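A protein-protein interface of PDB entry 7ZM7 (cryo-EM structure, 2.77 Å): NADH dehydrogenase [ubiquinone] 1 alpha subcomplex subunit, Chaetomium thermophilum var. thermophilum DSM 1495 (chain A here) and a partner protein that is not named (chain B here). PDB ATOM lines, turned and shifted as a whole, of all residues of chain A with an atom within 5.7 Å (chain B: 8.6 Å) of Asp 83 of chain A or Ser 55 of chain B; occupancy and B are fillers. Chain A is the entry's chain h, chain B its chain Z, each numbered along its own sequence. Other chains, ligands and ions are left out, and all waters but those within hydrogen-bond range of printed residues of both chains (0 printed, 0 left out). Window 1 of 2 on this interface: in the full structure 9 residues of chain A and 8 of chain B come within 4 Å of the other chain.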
ATOM      1  N   ARG A  56      16.790 -12.691  -0.466  1.00  0.00           N
ATOM      2  CA  ARG A  56      17.155 -12.287   0.887  1.00  0.00           C
ATOM      3  C   ARG A  56      15.926 -11.799   1.627  1.00  0.00           C
ATOM      4  O   ARG A  56      15.156 -11.006   1.087  1.00  0.00           O
ATOM      5  CB  ARG A  56      18.219 -11.201   0.870  1.00  0.00           C
ATOM      6  CG  ARG A  56      19.423 -11.589   0.107  1.00  0.00           C
ATOM      7  CD  ARG A  56      20.332 -10.442  -0.122  1.00  0.00           C
ATOM      8  NE  ARG A  56      21.461 -10.845  -0.938  1.00  0.00           N
ATOM      9  CZ  ARG A  56      22.435 -10.034  -1.304  1.00  0.00           C
ATOM     10  NH1 ARG A  56      22.433  -8.780  -0.900  1.00  0.00           N
ATOM     11  NH2 ARG A  56      23.418 -10.488  -2.055  1.00  0.00           N
ATOM     12  N   TRP A  77      22.611  -4.940   2.971  1.00  0.00           N
ATOM     13  CA  TRP A  77      22.559  -6.300   2.461  1.00  0.00           C
ATOM     14  C   TRP A  77      21.148  -6.665   2.011  1.00  0.00           C
ATOM     15  O   TRP A  77      20.956  -7.208   0.921  1.00  0.00           O
ATOM     16  CB  TRP A  77      23.069  -7.261   3.530  1.00  0.00           C
ATOM     17  CG  TRP A  77      23.121  -8.673   3.108  1.00  0.00           C
ATOM     18  CD1 TRP A  77      24.115  -9.286   2.416  1.00  0.00           C
ATOM     19  CD2 TRP A  77      22.138  -9.666   3.363  1.00  0.00           C
ATOM     20  NE1 TRP A  77      23.807 -10.602   2.220  1.00  0.00           N
ATOM     21  CE2 TRP A  77      22.594 -10.860   2.795  1.00  0.00           C
ATOM     22  CE3 TRP A  77      20.904  -9.659   4.009  1.00  0.00           C
ATOM     23  CZ2 TRP A  77      21.861 -12.033   2.854  1.00  0.00           C
ATOM     24  CZ3 TRP A  77      20.183 -10.823   4.068  1.00  0.00           C
ATOM     25  CH2 TRP A  77      20.659 -11.991   3.496  1.00  0.00           C
ATOM     26  N   TYR A  80      20.075  -5.377  -1.414  1.00  0.00           N
ATOM     27  CA  TYR A  80      20.881  -5.784  -2.552  1.00  0.00           C
ATOM     28  C   TYR A  80      21.878  -4.721  -2.942  1.00  0.00           C
ATOM     29  O   TYR A  80      22.305  -4.660  -4.091  1.00  0.00           O
ATOM     30  CB  TYR A  80      20.009  -6.177  -3.747  1.00  0.00           C
ATOM     31  CG  TYR A  80      19.188  -7.399  -3.469  1.00  0.00           C
ATOM     32  CD1 TYR A  80      17.931  -7.291  -2.889  1.00  0.00           C
ATOM     33  CD2 TYR A  80      19.671  -8.663  -3.755  1.00  0.00           C
ATOM     34  CE1 TYR A  80      17.180  -8.397  -2.609  1.00  0.00           C
ATOM     35  CE2 TYR A  80      18.917  -9.779  -3.479  1.00  0.00           C
ATOM     36  CZ  TYR A  80      17.668  -9.633  -2.910  1.00  0.00           C
ATOM     37  OH  TYR A  80      16.901 -10.721  -2.635  1.00  0.00           O
ATOM     38  N   GLN A  81      22.267  -3.886  -1.983  1.00  0.00           N
ATOM     39  CA  GLN A  81      23.245  -2.840  -2.223  1.00  0.00           C
ATOM     40  C   GLN A  81      24.661  -3.325  -1.987  1.00  0.00           C
ATOM     41  O   GLN A  81      25.606  -2.674  -2.428  1.00  0.00           O
ATOM     42  CB  GLN A  81      22.960  -1.638  -1.326  1.00  0.00           C
ATOM     43  CG  GLN A  81      23.481  -0.328  -1.849  1.00  0.00           C
ATOM     44  CD  GLN A  81      23.741   0.668  -0.747  1.00  0.00           C
ATOM     45  OE1 GLN A  81      23.883   0.304   0.412  1.00  0.00           O
ATOM     46  NE2 GLN A  81      23.737   1.940  -1.090  1.00  0.00           N
ATOM     47  N   VAL A  82      24.833  -4.420  -1.259  1.00  0.00           N
ATOM     48  CA  VAL A  82      26.103  -5.121  -1.159  1.00  0.00           C
ATOM     49  C   VAL A  82      25.811  -6.609  -1.276  1.00  0.00           C
ATOM     50  O   VAL A  82      24.682  -7.058  -1.090  1.00  0.00           O
ATOM     51  CB  VAL A  82      26.848  -4.831   0.158  1.00  0.00           C
ATOM     52  CG1 VAL A  82      27.189  -3.349   0.273  1.00  0.00           C
ATOM     53  CG2 VAL A  82      26.050  -5.302   1.341  1.00  0.00           C
ATOM     54  N   ASP A  83      26.843  -7.378  -1.603  1.00  0.00           N
ATOM     55  CA  ASP A  83      26.740  -8.828  -1.551  1.00  0.00           C
ATOM     56  C   ASP A  83      27.395  -9.429  -0.322  1.00  0.00           C
ATOM     57  O   ASP A  83      27.065 -10.559   0.037  1.00  0.00           O
ATOM     58  CB  ASP A  83      27.367  -9.466  -2.790  1.00  0.00           C
ATOM     59  CG  ASP A  83      26.627  -9.142  -4.043  1.00  0.00           C
ATOM     60  OD1 ASP A  83      25.390  -9.035  -3.987  1.00  0.00           O
ATOM     61  OD2 ASP A  83      27.282  -9.006  -5.094  1.00  0.00           O
ATOM     62  N   THR A  84      28.304  -8.716   0.326  1.00  0.00           N
ATOM     63  CA  THR A  84      28.938  -9.221   1.531  1.00  0.00           C
ATOM     64  C   THR A  84      28.115  -8.842   2.753  1.00  0.00           C
ATOM     65  O   THR A  84      27.851  -7.654   2.964  1.00  0.00           O
ATOM     66  CB  THR A  84      30.357  -8.696   1.653  1.00  0.00           C
ATOM     67  OG1 THR A  84      30.927  -9.144   2.885  1.00  0.00           O
ATOM     68  CG2 THR A  84      30.416  -7.178   1.560  1.00  0.00           C
ATOM     69  N   PRO A  85      27.666  -9.800   3.556  1.00  0.00           N
ATOM     70  CA  PRO A  85      26.882  -9.464   4.742  1.00  0.00           C
ATOM     71  C   PRO A  85      27.760  -8.866   5.823  1.00  0.00           C
ATOM     72  O   PRO A  85      28.986  -9.038   5.807  1.00  0.00           O
ATOM     73  CB  PRO A  85      26.295 -10.815   5.169  1.00  0.00           C
ATOM     74  CG  PRO A  85      27.195 -11.798   4.613  1.00  0.00           C
ATOM     75  CD  PRO A  85      27.793 -11.249   3.369  1.00  0.00           C
ATOM     76  N   ARG A  88      30.946 -10.563   7.417  1.00  0.00           N
ATOM     77  CA  ARG A  88      32.278 -10.668   6.841  1.00  0.00           C
ATOM     78  C   ARG A  88      32.763  -9.339   6.278  1.00  0.00           C
ATOM     79  O   ARG A  88      33.778  -9.319   5.574  1.00  0.00           O
ATOM     80  CB  ARG A  88      32.304 -11.728   5.741  1.00  0.00           C
ATOM     81  CG  ARG A  88      32.119 -13.149   6.235  1.00  0.00           C
ATOM     82  CD  ARG A  88      32.413 -14.147   5.133  1.00  0.00           C
ATOM     83  NE  ARG A  88      31.764 -13.781   3.879  1.00  0.00           N
ATOM     84  CZ  ARG A  88      30.480 -13.989   3.610  1.00  0.00           C
ATOM     85  NH1 ARG A  88      29.694 -14.565   4.508  1.00  0.00           N
ATOM     86  NH2 ARG A  88      29.980 -13.623   2.438  1.00  0.00           N
ATOM     87  N   TYR B  50      22.779 -14.078 -13.132  1.00  0.00           N
ATOM     88  CA  TYR B  50      23.253 -13.208 -14.199  1.00  0.00           C
ATOM     89  C   TYR B  50      22.855 -11.761 -14.025  1.00  0.00           C
ATOM     90  O   TYR B  50      23.627 -10.870 -14.371  1.00  0.00           O
ATOM     91  CB  TYR B  50      22.724 -13.682 -15.558  1.00  0.00           C
ATOM     92  CG  TYR B  50      23.282 -14.978 -16.049  1.00  0.00           C
ATOM     93  CD1 TYR B  50      24.386 -15.556 -15.457  1.00  0.00           C
ATOM     94  CD2 TYR B  50      22.704 -15.628 -17.125  1.00  0.00           C
ATOM     95  CE1 TYR B  50      24.887 -16.739 -15.922  1.00  0.00           C
ATOM     96  CE2 TYR B  50      23.207 -16.804 -17.592  1.00  0.00           C
ATOM     97  CZ  TYR B  50      24.289 -17.358 -16.988  1.00  0.00           C
ATOM     98  OH  TYR B  50      24.788 -18.540 -17.462  1.00  0.00           O
ATOM     99  N   ASN B  51      21.660 -11.504 -13.525  1.00  0.00           N
ATOM    100  CA  ASN B  51      21.071 -10.180 -13.571  1.00  0.00           C
ATOM    101  C   ASN B  51      21.437  -9.412 -12.321  1.00  0.00           C
ATOM    102  O   ASN B  51      21.161  -9.867 -11.210  1.00  0.00           O
ATOM    103  CB  ASN B  51      19.554 -10.266 -13.699  1.00  0.00           C
ATOM    104  CG  ASN B  51      18.958  -9.011 -14.237  1.00  0.00           C
ATOM    105  OD1 ASN B  51      18.463  -8.169 -13.492  1.00  0.00           O
ATOM    106  ND2 ASN B  51      19.003  -8.865 -15.548  1.00  0.00           N
ATOM    107  N   ARG B  52      22.044  -8.243 -12.515  1.00  0.00           N
ATOM    108  CA  ARG B  52      22.495  -7.388 -11.429  1.00  0.00           C
ATOM    109  C   ARG B  52      23.380  -8.165 -10.467  1.00  0.00           C
ATOM    110  O   ARG B  52      23.355  -7.944  -9.262  1.00  0.00           O
ATOM    111  CB  ARG B  52      21.311  -6.742 -10.704  1.00  0.00           C
ATOM    112  CG  ARG B  52      21.635  -5.490  -9.933  1.00  0.00           C
ATOM    113  CD  ARG B  52      20.401  -4.948  -9.266  1.00  0.00           C
ATOM    114  NE  ARG B  52      20.658  -3.732  -8.509  1.00  0.00           N
ATOM    115  CZ  ARG B  52      21.118  -3.713  -7.265  1.00  0.00           C
ATOM    116  NH1 ARG B  52      21.405  -4.834  -6.647  1.00  0.00           N
ATOM    117  NH2 ARG B  52      21.311  -2.573  -6.648  1.00  0.00           N
ATOM    118  N   ASN B  53      24.152  -9.093 -11.007  1.00  0.00           N
ATOM    119  CA  ASN B  53      25.017  -9.959 -10.217  1.00  0.00           C
ATOM    120  C   ASN B  53      26.444  -9.803 -10.706  1.00  0.00           C
ATOM    121  O   ASN B  53      26.736 -10.153 -11.864  1.00  0.00           O
ATOM    122  CB  ASN B  53      24.566 -11.413 -10.329  1.00  0.00           C
ATOM    123  CG  ASN B  53      25.213 -12.297  -9.305  1.00  0.00           C
ATOM    124  OD1 ASN B  53      25.302 -11.950  -8.133  1.00  0.00           O
ATOM    125  ND2 ASN B  53      25.688 -13.448  -9.747  1.00  0.00           N
ATOM    126  N   PRO B  54      27.370  -9.282  -9.897  1.00  0.00           N
ATOM    127  CA  PRO B  54      27.180  -8.827  -8.524  1.00  0.00           C
ATOM    128  C   PRO B  54      26.479  -7.484  -8.458  1.00  0.00           C
ATOM    129  O   PRO B  54      26.342  -6.817  -9.477  1.00  0.00           O
ATOM    130  CB  PRO B  54      28.606  -8.715  -8.008  1.00  0.00           C
ATOM    131  CG  PRO B  54      29.367  -8.363  -9.180  1.00  0.00           C
ATOM    132  CD  PRO B  54      28.760  -9.090 -10.328  1.00  0.00           C
ATOM    133  N   SER B  55      26.110  -7.060  -7.249  1.00  0.00           N
ATOM    134  CA  SER B  55      25.518  -5.716  -7.093  1.00  0.00           C
ATOM    135  C   SER B  55      26.572  -4.677  -7.466  1.00  0.00           C
ATOM    136  O   SER B  55      27.759  -5.040  -7.529  1.00  0.00           O
ATOM    137  CB  SER B  55      25.029  -5.553  -5.693  1.00  0.00           C
ATOM    138  OG  SER B  55      26.104  -5.641  -4.773  1.00  0.00           O
ATOM    139  N   PRO B  56      26.212  -3.397  -7.704  1.00  0.00           N
ATOM    140  CA  PRO B  56      27.209  -2.378  -7.968  1.00  0.00           C
ATOM    141  C   PRO B  56      28.060  -2.139  -6.713  1.00  0.00           C
ATOM    142  O   PRO B  56      29.161  -1.652  -6.854  1.00  0.00           O
ATOM    143  CB  PRO B  56      26.405  -1.176  -8.455  1.00  0.00           C
ATOM    144  CG  PRO B  56      25.038  -1.736  -8.772  1.00  0.00           C
ATOM    145  CD  PRO B  56      24.851  -2.884  -7.810  1.00  0.00           C
ATOM    146  N   GLY B  57      27.537  -2.483  -5.534  1.00  0.00           N
ATOM    147  CA  GLY B  57      28.298  -2.323  -4.285  1.00  0.00           C
ATOM    148  C   GLY B  57      29.458  -3.287  -4.168  1.00  0.00           C
ATOM    149  O   GLY B  57      30.387  -2.982  -3.421  1.00  0.00           O
ATOM    150  N   ASP B  58      29.393  -4.424  -4.858  1.00  0.00           N
ATOM    151  CA  ASP B  58      30.529  -5.382  -4.857  1.00  0.00           C
ATOM    152  C   ASP B  58      31.358  -5.276  -6.141  1.00  0.00           C
ATOM    153  O   ASP B  58      32.351  -6.016  -6.243  1.00  0.00           O
ATOM    154  CB  ASP B  58      30.095  -6.800  -4.485  1.00  0.00           C
ATOM    155  CG  ASP B  58      29.945  -7.007  -2.987  1.00  0.00           C
ATOM    156  OD1 ASP B  58      29.476  -6.073  -2.303  1.00  0.00           O
ATOM    157  OD2 ASP B  58      30.320  -8.094  -2.509  1.00  0.00           O
ATOM    158  N   ASN B  59      30.989  -4.406  -7.082  1.00  0.00           N
ATOM    159  CA  ASN B  59      31.866  -4.189  -8.260  1.00  0.00           C
ATOM    160  C   ASN B  59      33.181  -3.662  -7.693  1.00  0.00           C
ATOM    161  O   ASN B  59      33.126  -2.727  -6.876  1.00  0.00           O
ATOM    162  CB  ASN B  59      31.257  -3.166  -9.211  1.00  0.00           C
ATOM    163  CG  ASN B  59      30.146  -3.720 -10.077  1.00  0.00           C
ATOM    164  OD1 ASN B  59      29.935  -4.929 -10.133  1.00  0.00           O
ATOM    165  ND2 ASN B  59      29.441  -2.841 -10.770  1.00  0.00           N
ATOM    166  N   PRO B  60      34.359  -4.209  -8.057  1.00  0.00           N
ATOM    167  CA  PRO B  60      35.616  -3.787  -7.439  1.00  0.00           C
ATOM    168  C   PRO B  60      35.960  -2.305  -7.667  1.00  0.00           C
ATOM    169  O   PRO B  60      36.063  -1.939  -8.817  1.00  0.00           O
ATOM    170  CB  PRO B  60      36.652  -4.704  -8.081  1.00  0.00           C
ATOM    171  CG  PRO B  60      35.852  -5.886  -8.574  1.00  0.00           C
ATOM    172  CD  PRO B  60      34.541  -5.283  -9.029  1.00  0.00           C
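The guanidinium group of Arg 52 of chain B is in hydrogen-bond range of the backbone carbonyl oxygen of Tyr 80 of chain A, 2.7 Å away. OD2 of Asp 83 of chain A is in hydrogen-bond range of N of Ser 55 of chain B (3.1 Å). OD1 of Asp 58 of chain B lies within hydrogen-bond range of N of Asp 83 of chain A, 3.0 Å away.
Among the printed residues, pairs that only touch across the chains: Asp 83 of chain A with Pro 54 of chain B (3.2 Å), Tyr 80 of chain A with Ser 55 of chain B (3.3 Å), Gln 81 of chain A with Gly 57 of chain B (3.3 Å), Thr 84 of chain A with Asp 58 of chain B (3.5 Å), Val 82 of chain A with Ser 55 of chain B (3.6 Å), Val 82 of chain A with Asp 58 of chain B (3.7 Å) and Gln 81 of chain A with Ser 55 of chain B (3.8 Å).
The backbone carbonyl oxygen (O) of Ser 55 of chain B sits close to the side-chain amide oxygen (OD1) of Asn 59 of chain B (3.4 Å). N of Arg 56 of chain A lies within hydrogen-bond range of OH of Tyr 80 of chain A. NH1 of Arg 56 of chain A is in hydrogen-bond range of O of Val 82 of chain A, 2.8 Å away. The guanidinium group of Arg 56 of chain A is in salt-bridge range of the side-chain carboxylate of Asp 83 of chain A, at 3.1 Å.
Of the 9 printed residues of chain A, 5 touch a printed residue of chain B. Printed residues of chain A that touch a printed residue of chain B: Tyr 80, Gln 81, Val 82, Asp 83 and Thr 84. Hydrophobic or aromatic side chains of chain A that line the printed part of chain B: Tyr 80 and Val 82. Of the 11 printed residues of chain B, 5 touch a printed residue of chain A. Printed residues of chain B that touch a printed residue of chain A: Arg 52, Pro 54, Ser 55, Gly 57 and Asp 58. Hydrophobic or aromatic side chains of chain B that line the printed part of chain A: Pro 54. Among the printed residues, no Asp or Glu carboxylate lies within 4 Å of a Lys or Arg side-chain nitrogen of the other chain.
Of the printed residues of chain B, Asp 83 of chain A touches Pro 54, Ser 55 and Asp 58. Ser 55 of chain B touches four residues of chain A. Val 82 of chain A touches just these residues of chain B: Ser 55 and Asp 58. Of the printed residues of chain A, Asp 58 of chain B touches Val 82, Asp 83 and Thr 84. Of the printed residues of chain A, Pro 54 of chain B touches Asp 83 (3.2 Å). Printed residues of chain A within 4 Å of Gly 57 of chain B: Gln 81. The nearest printed residue of chain A that does not touch Ser 55 of chain B is Arg 56 of chain A (6.2 Å).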
